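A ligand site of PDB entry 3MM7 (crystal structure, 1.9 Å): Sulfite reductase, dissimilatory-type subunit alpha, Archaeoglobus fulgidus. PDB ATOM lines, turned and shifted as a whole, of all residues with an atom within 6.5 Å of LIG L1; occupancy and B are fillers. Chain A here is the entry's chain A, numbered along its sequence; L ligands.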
ATOM      1  N   CYS A 176      -0.624  -5.696  27.658  1.00  0.00           N
ATOM      2  CA  CYS A 176      -0.128  -5.234  26.359  1.00  0.00           C
ATOM      3  C   CYS A 176       0.680  -6.337  25.750  1.00  0.00           C
ATOM      4  O   CYS A 176       1.065  -7.317  26.411  1.00  0.00           O
ATOM      5  CB  CYS A 176       0.659  -3.969  26.462  1.00  0.00           C
ATOM      6  SG  CYS A 176       2.342  -4.304  26.858  1.00  0.00           S
ATOM      7  N   MET A 177       0.920  -6.205  24.460  1.00  0.00           N
ATOM      8  CA  MET A 177       1.642  -7.281  23.709  1.00  0.00           C
ATOM      9  C   MET A 177       2.932  -7.641  24.347  1.00  0.00           C
ATOM     10  O   MET A 177       3.348  -8.758  24.270  1.00  0.00           O
ATOM     11  CB  MET A 177       1.836  -6.945  22.236  1.00  0.00           C
ATOM     12  CG  MET A 177       2.730  -5.716  21.947  1.00  0.00           C
ATOM     13  SD  MET A 177       2.308  -5.193  20.228  1.00  0.00           S
ATOM     14  CE  MET A 177       3.653  -4.096  20.004  1.00  0.00           C
ATOM     15  N   GLY A 178       3.608  -6.661  24.971  1.00  0.00           N
ATOM     16  CA  GLY A 178       4.709  -7.018  25.684  1.00  0.00           C
ATOM     17  C   GLY A 178       5.763  -7.739  24.818  1.00  0.00           C
ATOM     18  O   GLY A 178       5.853  -7.493  23.636  1.00  0.00           O
ATOM     19  N   PRO A 179       6.502  -8.674  25.432  1.00  0.00           N
ATOM     20  CA  PRO A 179       7.729  -9.156  24.796  1.00  0.00           C
ATOM     21  C   PRO A 179       7.413 -10.028  23.626  1.00  0.00           C
ATOM     22  O   PRO A 179       8.285 -10.295  22.866  1.00  0.00           O
ATOM     23  CB  PRO A 179       8.487  -9.904  25.929  1.00  0.00           C
ATOM     24  CG  PRO A 179       7.293 -10.402  26.874  1.00  0.00           C
ATOM     25  CD  PRO A 179       6.339  -9.199  26.806  1.00  0.00           C
ATOM     26  N   CYS A 182       7.345  -6.600  21.159  1.00  0.00           N
ATOM     27  CA  CYS A 182       7.774  -5.241  21.392  1.00  0.00           C
ATOM     28  C   CYS A 182       9.153  -5.218  22.060  1.00  0.00           C
ATOM     29  O   CYS A 182       9.381  -5.941  23.031  1.00  0.00           O
ATOM     30  CB  CYS A 182       6.657  -4.531  22.231  1.00  0.00           C
ATOM     31  SG  CYS A 182       7.125  -2.759  22.549  1.00  0.00           S
ATOM     32  N   GLU A 183      10.072  -4.391  21.547  1.00  0.00           N
ATOM     33  CA  GLU A 183      11.417  -4.286  22.077  1.00  0.00           C
ATOM     34  C   GLU A 183      11.559  -3.389  23.287  1.00  0.00           C
ATOM     35  O   GLU A 183      12.664  -3.288  23.861  1.00  0.00           O
ATOM     36  CB  GLU A 183      12.450  -3.861  20.991  1.00  0.00           C
ATOM     37  CG  GLU A 183      12.321  -2.428  20.493  1.00  0.00           C
ATOM     38  CD  GLU A 183      11.259  -2.188  19.446  1.00  0.00           C
ATOM     39  OE1 GLU A 183      10.263  -2.966  19.276  1.00  0.00           O
ATOM     40  OE2 GLU A 183      11.356  -1.143  18.794  1.00  0.00           O
ATOM     41  N   PHE A 184      10.492  -2.733  23.728  1.00  0.00           N
ATOM     42  CA  PHE A 184      10.662  -1.869  24.947  1.00  0.00           C
ATOM     43  C   PHE A 184      10.195  -2.515  26.283  1.00  0.00           C
ATOM     44  O   PHE A 184      10.186  -1.867  27.342  1.00  0.00           O
ATOM     45  CB  PHE A 184       9.945  -0.479  24.850  1.00  0.00           C
ATOM     46  CG  PHE A 184       9.997   0.233  23.514  1.00  0.00           C
ATOM     47  CD1 PHE A 184      11.130   0.209  22.677  1.00  0.00           C
ATOM     48  CD2 PHE A 184       8.946   1.102  23.216  1.00  0.00           C
ATOM     49  CE1 PHE A 184      11.134   1.014  21.465  1.00  0.00           C
ATOM     50  CE2 PHE A 184       8.892   1.853  22.078  1.00  0.00           C
ATOM     51  CZ  PHE A 184       9.989   1.802  21.172  1.00  0.00           C
ATOM     52  N   ALA A 185       9.856  -3.786  26.276  1.00  0.00           N
ATOM     53  CA  ALA A 185       9.034  -4.379  27.354  1.00  0.00           C
ATOM     54  C   ALA A 185       9.942  -4.690  28.460  1.00  0.00           C
ATOM     55  O   ALA A 185      11.014  -5.190  28.229  1.00  0.00           O
ATOM     56  CB  ALA A 185       8.386  -5.665  26.857  1.00  0.00           C
ATOM     57  N   CYS A 186       9.531  -4.356  29.682  1.00  0.00           N
ATOM     58  CA  CYS A 186      10.450  -4.479  30.800  1.00  0.00           C
ATOM     59  C   CYS A 186      10.157  -5.718  31.590  1.00  0.00           C
ATOM     60  O   CYS A 186      10.884  -6.020  32.444  1.00  0.00           O
ATOM     61  CB  CYS A 186      10.438  -3.238  31.673  1.00  0.00           C
ATOM     62  SG  CYS A 186      11.004  -1.826  30.795  1.00  0.00           S
ATOM     63  N   THR A 189       4.697  -9.288  30.305  1.00  0.00           N
ATOM     64  CA  THR A 189       3.311  -8.890  30.512  1.00  0.00           C
ATOM     65  C   THR A 189       2.315 -10.039  30.323  1.00  0.00           C
ATOM     66  O   THR A 189       1.396 -10.260  31.192  1.00  0.00           O
ATOM     67  CB  THR A 189       2.846  -7.665  29.638  1.00  0.00           C
ATOM     68  OG1 THR A 189       2.999  -7.936  28.272  1.00  0.00           O
ATOM     69  CG2 THR A 189       3.664  -6.311  30.008  1.00  0.00           C
ATOM     70  N   CYS A 217      -1.773  -5.014  32.909  1.00  0.00           N
ATOM     71  CA  CYS A 217      -0.300  -5.060  32.946  1.00  0.00           C
ATOM     72  C   CYS A 217       0.307  -4.390  31.732  1.00  0.00           C
ATOM     73  O   CYS A 217       0.125  -4.814  30.614  1.00  0.00           O
ATOM     74  CB  CYS A 217       0.309  -6.470  33.213  1.00  0.00           C
ATOM     75  SG  CYS A 217      -0.747  -7.649  34.172  1.00  0.00           S
ATOM     76  N   ALA A 218       1.097  -3.358  31.987  1.00  0.00           N
ATOM     77  CA  ALA A 218       1.750  -2.718  30.865  1.00  0.00           C
ATOM     78  C   ALA A 218       3.235  -2.825  30.903  1.00  0.00           C
ATOM     79  O   ALA A 218       3.883  -2.621  31.957  1.00  0.00           O
ATOM     80  CB  ALA A 218       1.255  -1.282  30.668  1.00  0.00           C
ATOM     81  N   GLY A 219       3.759  -3.059  29.688  1.00  0.00           N
ATOM     82  CA  GLY A 219       5.107  -3.573  29.548  1.00  0.00           C
ATOM     83  C   GLY A 219       6.072  -2.458  29.857  1.00  0.00           C
ATOM     84  O   GLY A 219       7.179  -2.717  30.299  1.00  0.00           O
ATOM     85  N   CYS A 220       5.590  -1.225  29.772  1.00  0.00           N
ATOM     86  CA  CYS A 220       6.576  -0.070  29.756  1.00  0.00           C
ATOM     87  C   CYS A 220       5.854   1.216  30.032  1.00  0.00           C
ATOM     88  O   CYS A 220       4.613   1.207  30.002  1.00  0.00           O
ATOM     89  CB  CYS A 220       7.328  -0.082  28.313  1.00  0.00           C
ATOM     90  SG  CYS A 220       6.760   0.843  27.096  1.00  0.00           S
ATOM     91  N   PRO A 221       6.577   2.364  30.289  1.00  0.00           N
ATOM     92  CA  PRO A 221       5.563   3.390  30.620  1.00  0.00           C
ATOM     93  C   PRO A 221       4.564   4.005  29.537  1.00  0.00           C
ATOM     94  O   PRO A 221       3.696   4.859  29.898  1.00  0.00           O
ATOM     95  CB  PRO A 221       6.354   4.514  31.183  1.00  0.00           C
ATOM     96  CG  PRO A 221       7.841   3.968  31.417  1.00  0.00           C
ATOM     97  CD  PRO A 221       7.860   2.574  30.968  1.00  0.00           C
ATOM     98  N   ASN A 222       4.701   3.638  28.267  1.00  0.00           N
ATOM     99  CA  ASN A 222       3.801   4.172  27.244  1.00  0.00           C
ATOM    100  C   ASN A 222       2.374   3.770  27.584  1.00  0.00           C
ATOM    101  O   ASN A 222       1.437   4.267  26.954  1.00  0.00           O
ATOM    102  CB  ASN A 222       4.135   3.482  25.913  1.00  0.00           C
ATOM    103  CG  ASN A 222       5.347   4.122  25.224  1.00  0.00           C
ATOM    104  OD1 ASN A 222       5.661   5.309  25.441  1.00  0.00           O
ATOM    105  ND2 ASN A 222       5.990   3.345  24.369  1.00  0.00           N
ATOM    106  N   ASP A 223       2.225   2.772  28.481  1.00  0.00           N
ATOM    107  CA  ASP A 223       0.862   2.125  28.824  1.00  0.00           C
ATOM    108  C   ASP A 223      -0.190   1.786  27.742  1.00  0.00           C
ATOM    109  O   ASP A 223      -1.375   2.319  27.818  1.00  0.00           O
ATOM    110  CB  ASP A 223       0.143   3.151  29.760  1.00  0.00           C
ATOM    111  CG  ASP A 223      -0.630   2.532  30.918  1.00  0.00           C
ATOM    112  OD1 ASP A 223      -1.022   1.323  30.830  1.00  0.00           O
ATOM    113  OD2 ASP A 223      -1.058   3.308  31.846  1.00  0.00           O
ATOM    114  N   CYS A 224       0.129   0.882  26.820  1.00  0.00           N
ATOM    115  CA  CYS A 224      -0.694   0.635  25.603  1.00  0.00           C
ATOM    116  C   CYS A 224      -1.905  -0.178  25.981  1.00  0.00           C
ATOM    117  O   CYS A 224      -2.746  -0.664  25.051  1.00  0.00           O
ATOM    118  CB  CYS A 224       0.162  -0.101  24.572  1.00  0.00           C
ATOM    119  SG  CYS A 224       1.793   0.857  24.206  1.00  0.00           S
ATOM    120  N   VAL A 225      -2.125  -0.377  27.294  1.00  0.00           N
ATOM    121  CA  VAL A 225      -3.448  -1.017  27.729  1.00  0.00           C
ATOM    122  C   VAL A 225      -4.249  -0.062  28.567  1.00  0.00           C
ATOM    123  O   VAL A 225      -5.380  -0.341  28.951  1.00  0.00           O
ATOM    124  CB  VAL A 225      -3.313  -2.407  28.484  1.00  0.00           C
ATOM    125  CG1 VAL A 225      -3.082  -3.439  27.461  1.00  0.00           C
ATOM    126  CG2 VAL A 225      -2.249  -2.365  29.606  1.00  0.00           C
ATOM    127  N   MET A 290       9.663   7.514  28.645  1.00  0.00           N
ATOM    128  CA  MET A 290      10.070   7.049  27.318  1.00  0.00           C
ATOM    129  C   MET A 290      10.551   7.944  26.132  1.00  0.00           C
ATOM    130  O   MET A 290      11.236   7.445  25.321  1.00  0.00           O
ATOM    131  CB  MET A 290       8.952   6.057  26.805  1.00  0.00           C
ATOM    132  CG  MET A 290       8.785   4.724  27.821  1.00  0.00           C
ATOM    133  SD  MET A 290      10.127   3.538  27.783  1.00  0.00           S
ATOM    134  CE  MET A 290       9.684   2.816  26.120  1.00  0.00           C
ATOM    135  N   ASN A 294      11.214   5.855  22.333  1.00  0.00           N
ATOM    136  CA  ASN A 294      10.188   6.131  21.295  1.00  0.00           C
ATOM    137  C   ASN A 294      10.728   6.808  19.989  1.00  0.00           C
ATOM    138  O   ASN A 294      10.465   6.302  18.903  1.00  0.00           O
ATOM    139  CB  ASN A 294       8.968   6.925  21.862  1.00  0.00           C
ATOM    140  CG  ASN A 294       8.175   6.177  22.982  1.00  0.00           C
ATOM    141  OD1 ASN A 294       8.360   4.984  23.228  1.00  0.00           O
ATOM    142  ND2 ASN A 294       7.361   6.920  23.703  1.00  0.00           N
HETATM  143 FE1  LIG L   1       5.383  -0.591  26.386  1.00  0.00          FE
HETATM  144 FE2  LIG L   1       3.358  -0.622  24.750  1.00  0.00          FE
HETATM  145 FE3  LIG L   1       5.400  -2.087  24.047  1.00  0.00          FE
HETATM  146 FE4  LIG L   1       3.797  -2.570  26.068  1.00  0.00          FE
HETATM  147  S1  LIG L   1       3.162  -2.765  23.760  1.00  0.00           S
HETATM  148  S2  LIG L   1       6.067  -2.683  26.179  1.00  0.00           S
HETATM  149  S3  LIG L   1       3.158  -0.724  27.039  1.00  0.00           S
HETATM  150  S4  LIG L   1       5.465   0.189  24.267  1.00  0.00           S
HETATM  151 FE1  LG2 L   2       1.221   1.918  21.905  1.00  0.00          FE
HETATM  152  C1  LG2 L   2       4.071   2.908  20.793  1.00  0.00           C
HETATM  153  C2  LG2 L   2       1.631  -1.060  19.988  1.00  0.00           C
HETATM  154  C3  LG2 L   2      -1.649   1.335  22.494  1.00  0.00           C
HETATM  155  C4  LG2 L   2       0.776   4.842  23.624  1.00  0.00           C
HETATM  156  N1  LG2 L   2       2.598   1.058  20.723  1.00  0.00           N
HETATM  157  C5  LG2 L   2       3.847   1.618  20.355  1.00  0.00           C
HETATM  158  C6  LG2 L   2       4.880   0.855  19.536  1.00  0.00           C
HETATM  159  C7  LG2 L   2       5.385   1.571  18.271  1.00  0.00           C
HETATM  160  C8  LG2 L   2       5.918  -0.021  20.380  1.00  0.00           C
HETATM  161  C9  LG2 L   2       7.069  -0.680  19.698  1.00  0.00           C
HETATM  162  O1  LG2 L   2       6.771  -1.554  18.878  1.00  0.00           O
HETATM  163  O2  LG2 L   2       8.221  -0.255  20.028  1.00  0.00           O
HETATM  164  C10 LG2 L   2       3.900  -0.257  19.059  1.00  0.00           C
HETATM  165  C11 LG2 L   2       3.613   0.204  17.622  1.00  0.00           C
HETATM  166  C12 LG2 L   2       2.546   1.320  17.599  1.00  0.00           C
HETATM  167  C13 LG2 L   2       2.400   2.062  16.309  1.00  0.00           C
HETATM  168  O3  LG2 L   2       1.338   1.921  15.634  1.00  0.00           O
HETATM  169  O4  LG2 L   2       3.337   2.818  16.014  1.00  0.00           O
HETATM  170  C14 LG2 L   2       2.722  -0.040  20.009  1.00  0.00           C
HETATM  171  N2  LG2 L   2       0.146   0.411  21.258  1.00  0.00           N
HETATM  172  C15 LG2 L   2       0.488  -0.664  20.669  1.00  0.00           C
HETATM  173  C16 LG2 L   2      -0.714  -1.769  20.639  1.00  0.00           C
HETATM  174  C17 LG2 L   2      -0.262  -2.586  19.383  1.00  0.00           C
HETATM  175  C18 LG2 L   2      -0.536  -2.554  21.942  1.00  0.00           C
HETATM  176  C19 LG2 L   2      -1.527  -3.819  22.082  1.00  0.00           C
HETATM  177  O5  LG2 L   2      -1.253  -4.774  22.759  1.00  0.00           O
HETATM  178  O6  LG2 L   2      -2.423  -3.790  21.276  1.00  0.00           O
HETATM  179  C20 LG2 L   2      -1.636  -0.778  20.952  1.00  0.00           C
HETATM  180  C21 LG2 L   2      -2.239  -0.401  19.608  1.00  0.00           C
HETATM  181  C22 LG2 L   2      -3.484   0.505  19.579  1.00  0.00           C
HETATM  182  C23 LG2 L   2      -4.113   0.771  18.229  1.00  0.00           C
HETATM  183  O7  LG2 L   2      -4.763  -0.121  17.507  1.00  0.00           O
HETATM  184  O8  LG2 L   2      -3.994   1.968  17.860  1.00  0.00           O
HETATM  185  C24 LG2 L   2      -1.037   0.540  21.617  1.00  0.00           C
HETATM  186  N3  LG2 L   2      -0.213   2.959  22.788  1.00  0.00           N
HETATM  187  C25 LG2 L   2      -1.475   2.450  23.034  1.00  0.00           C
HETATM  188  C26 LG2 L   2      -2.427   3.132  23.963  1.00  0.00           C
HETATM  189  C27 LG2 L   2      -3.623   2.666  24.771  1.00  0.00           C
HETATM  190  C28 LG2 L   2      -4.854   3.371  24.075  1.00  0.00           C
HETATM  191  O9  LG2 L   2      -4.707   4.325  23.245  1.00  0.00           O
HETATM  192  O10 LG2 L   2      -6.001   3.066  24.452  1.00  0.00           O
HETATM  193  C29 LG2 L   2      -1.618   4.315  24.248  1.00  0.00           C
HETATM  194  C30 LG2 L   2      -1.908   5.339  25.372  1.00  0.00           C
HETATM  195  C31 LG2 L   2      -2.843   6.441  24.697  1.00  0.00           C
HETATM  196  C32 LG2 L   2      -2.525   7.729  25.417  1.00  0.00           C
HETATM  197  O11 LG2 L   2      -3.348   8.541  25.817  1.00  0.00           O
HETATM  198  O12 LG2 L   2      -1.333   7.874  25.628  1.00  0.00           O
HETATM  199  C33 LG2 L   2      -0.316   3.964  23.561  1.00  0.00           C
HETATM  200  N4  LG2 L   2       2.240   3.560  22.226  1.00  0.00           N
HETATM  201  C34 LG2 L   2       1.845   4.573  22.894  1.00  0.00           C
HETATM  202  C35 LG2 L   2       3.019   5.621  23.027  1.00  0.00           C
HETATM  203  C36 LG2 L   2       2.740   7.130  23.259  1.00  0.00           C
HETATM  204  C37 LG2 L   2       2.380   8.240  22.250  1.00  0.00           C
HETATM  205  C38 LG2 L   2       2.817   9.670  22.720  1.00  0.00           C
HETATM  206  O13 LG2 L   2       3.241  10.400  21.820  1.00  0.00           O
HETATM  207  O14 LG2 L   2       2.456  10.201  23.834  1.00  0.00           O
HETATM  208  C39 LG2 L   2       4.002   5.095  22.054  1.00  0.00           C
HETATM  209  C40 LG2 L   2       5.155   5.989  21.460  1.00  0.00           C
HETATM  210  C41 LG2 L   2       5.098   6.113  19.955  1.00  0.00           C
HETATM  211  O15 LG2 L   2       4.228   6.844  19.348  1.00  0.00           O
HETATM  212  O16 LG2 L   2       5.988   5.454  19.392  1.00  0.00           O
HETATM  213  C42 LG2 L   2       3.362   3.789  21.597  1.00  0.00           C
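S3 of LIG L1 sits close to N of Cys 220 (3.7 Å).
An iron atom (FE1) of LIG L1 is bound by the side-chain sulfur (SG) of Cys 220 (2.1 Å).
S3 of LIG L1 lies close to N of Cys 224, at 3.4 Å.
An iron atom (FE2) of LIG L1 is bound by the side-chain sulfur (SG) of Cys 224, 2.2 Å away.
FE3 of LIG L1 is bound by SG of Cys 182 (2.4 Å).
The side-chain sulfur (SG) of Cys 176 is bound to an iron atom (FE4) of LIG L1, 2.4 Å away.
A sulfur (S4) of LIG L1 lies close to the side-chain amide nitrogen (ND2) of Asn 222 (3.2 Å).
N of Gly 219 lies close to S3 of LIG L1 (3.6 Å).
An iron atom (FE1) of LG2 L2 is bound by the side-chain sulfur (SG) of Cys 224.
The side-chain sulfur (SG) of Cys 182 sits close to an oxygen (O2) of LG2 L2, 3.7 Å away.
The backbone NH (N) of Met 177 lies within hydrogen-bond range of an oxygen (O5) of LG2 L2.
N of Asn 222 lies close to SG of Cys 220, at 3.7 Å.
The side-chain sulfur (SG) of Cys 182 sits close to the backbone NH (N) of Phe 184 (3.6 Å).
The side-chain sulfur of Cys 176 lies close to the backbone NH of Gly 219, 3.4 Å away.
SG of Cys 176 lies close to N of Gly 178 (3.3 Å).
O of Cys 176 sits at hydrogen-bond distance from OG1 of Thr 189 (2.8 Å).
The backbone carbonyl oxygen of Cys 217 sits at hydrogen-bond distance from the backbone NH of Cys 176, 3.2 Å away.
The side-chain amide oxygen (OD1) of Asn 222 sits at hydrogen-bond distance from the side-chain amide nitrogen (ND2) of Asn 294, at 2.9 Å.
O of Gly 219 lies within hydrogen-bond range of N of Cys 186.
Merely in contact with LIG L1: Met 177 (3.5 Å), Ala 185 (3.6 Å), Phe 184 (3.7 Å) and Asp 223 (3.9 Å).
Hydrophobic or aromatic side chains that line LIG L1: Met 177, Phe 184 and Ala 185.
Of the 21 residues printed, 10 come within 4 Å of LIG L1.
The nearest printed residue that does not touch LIG L1 is Gly 178 (4.1 Å).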
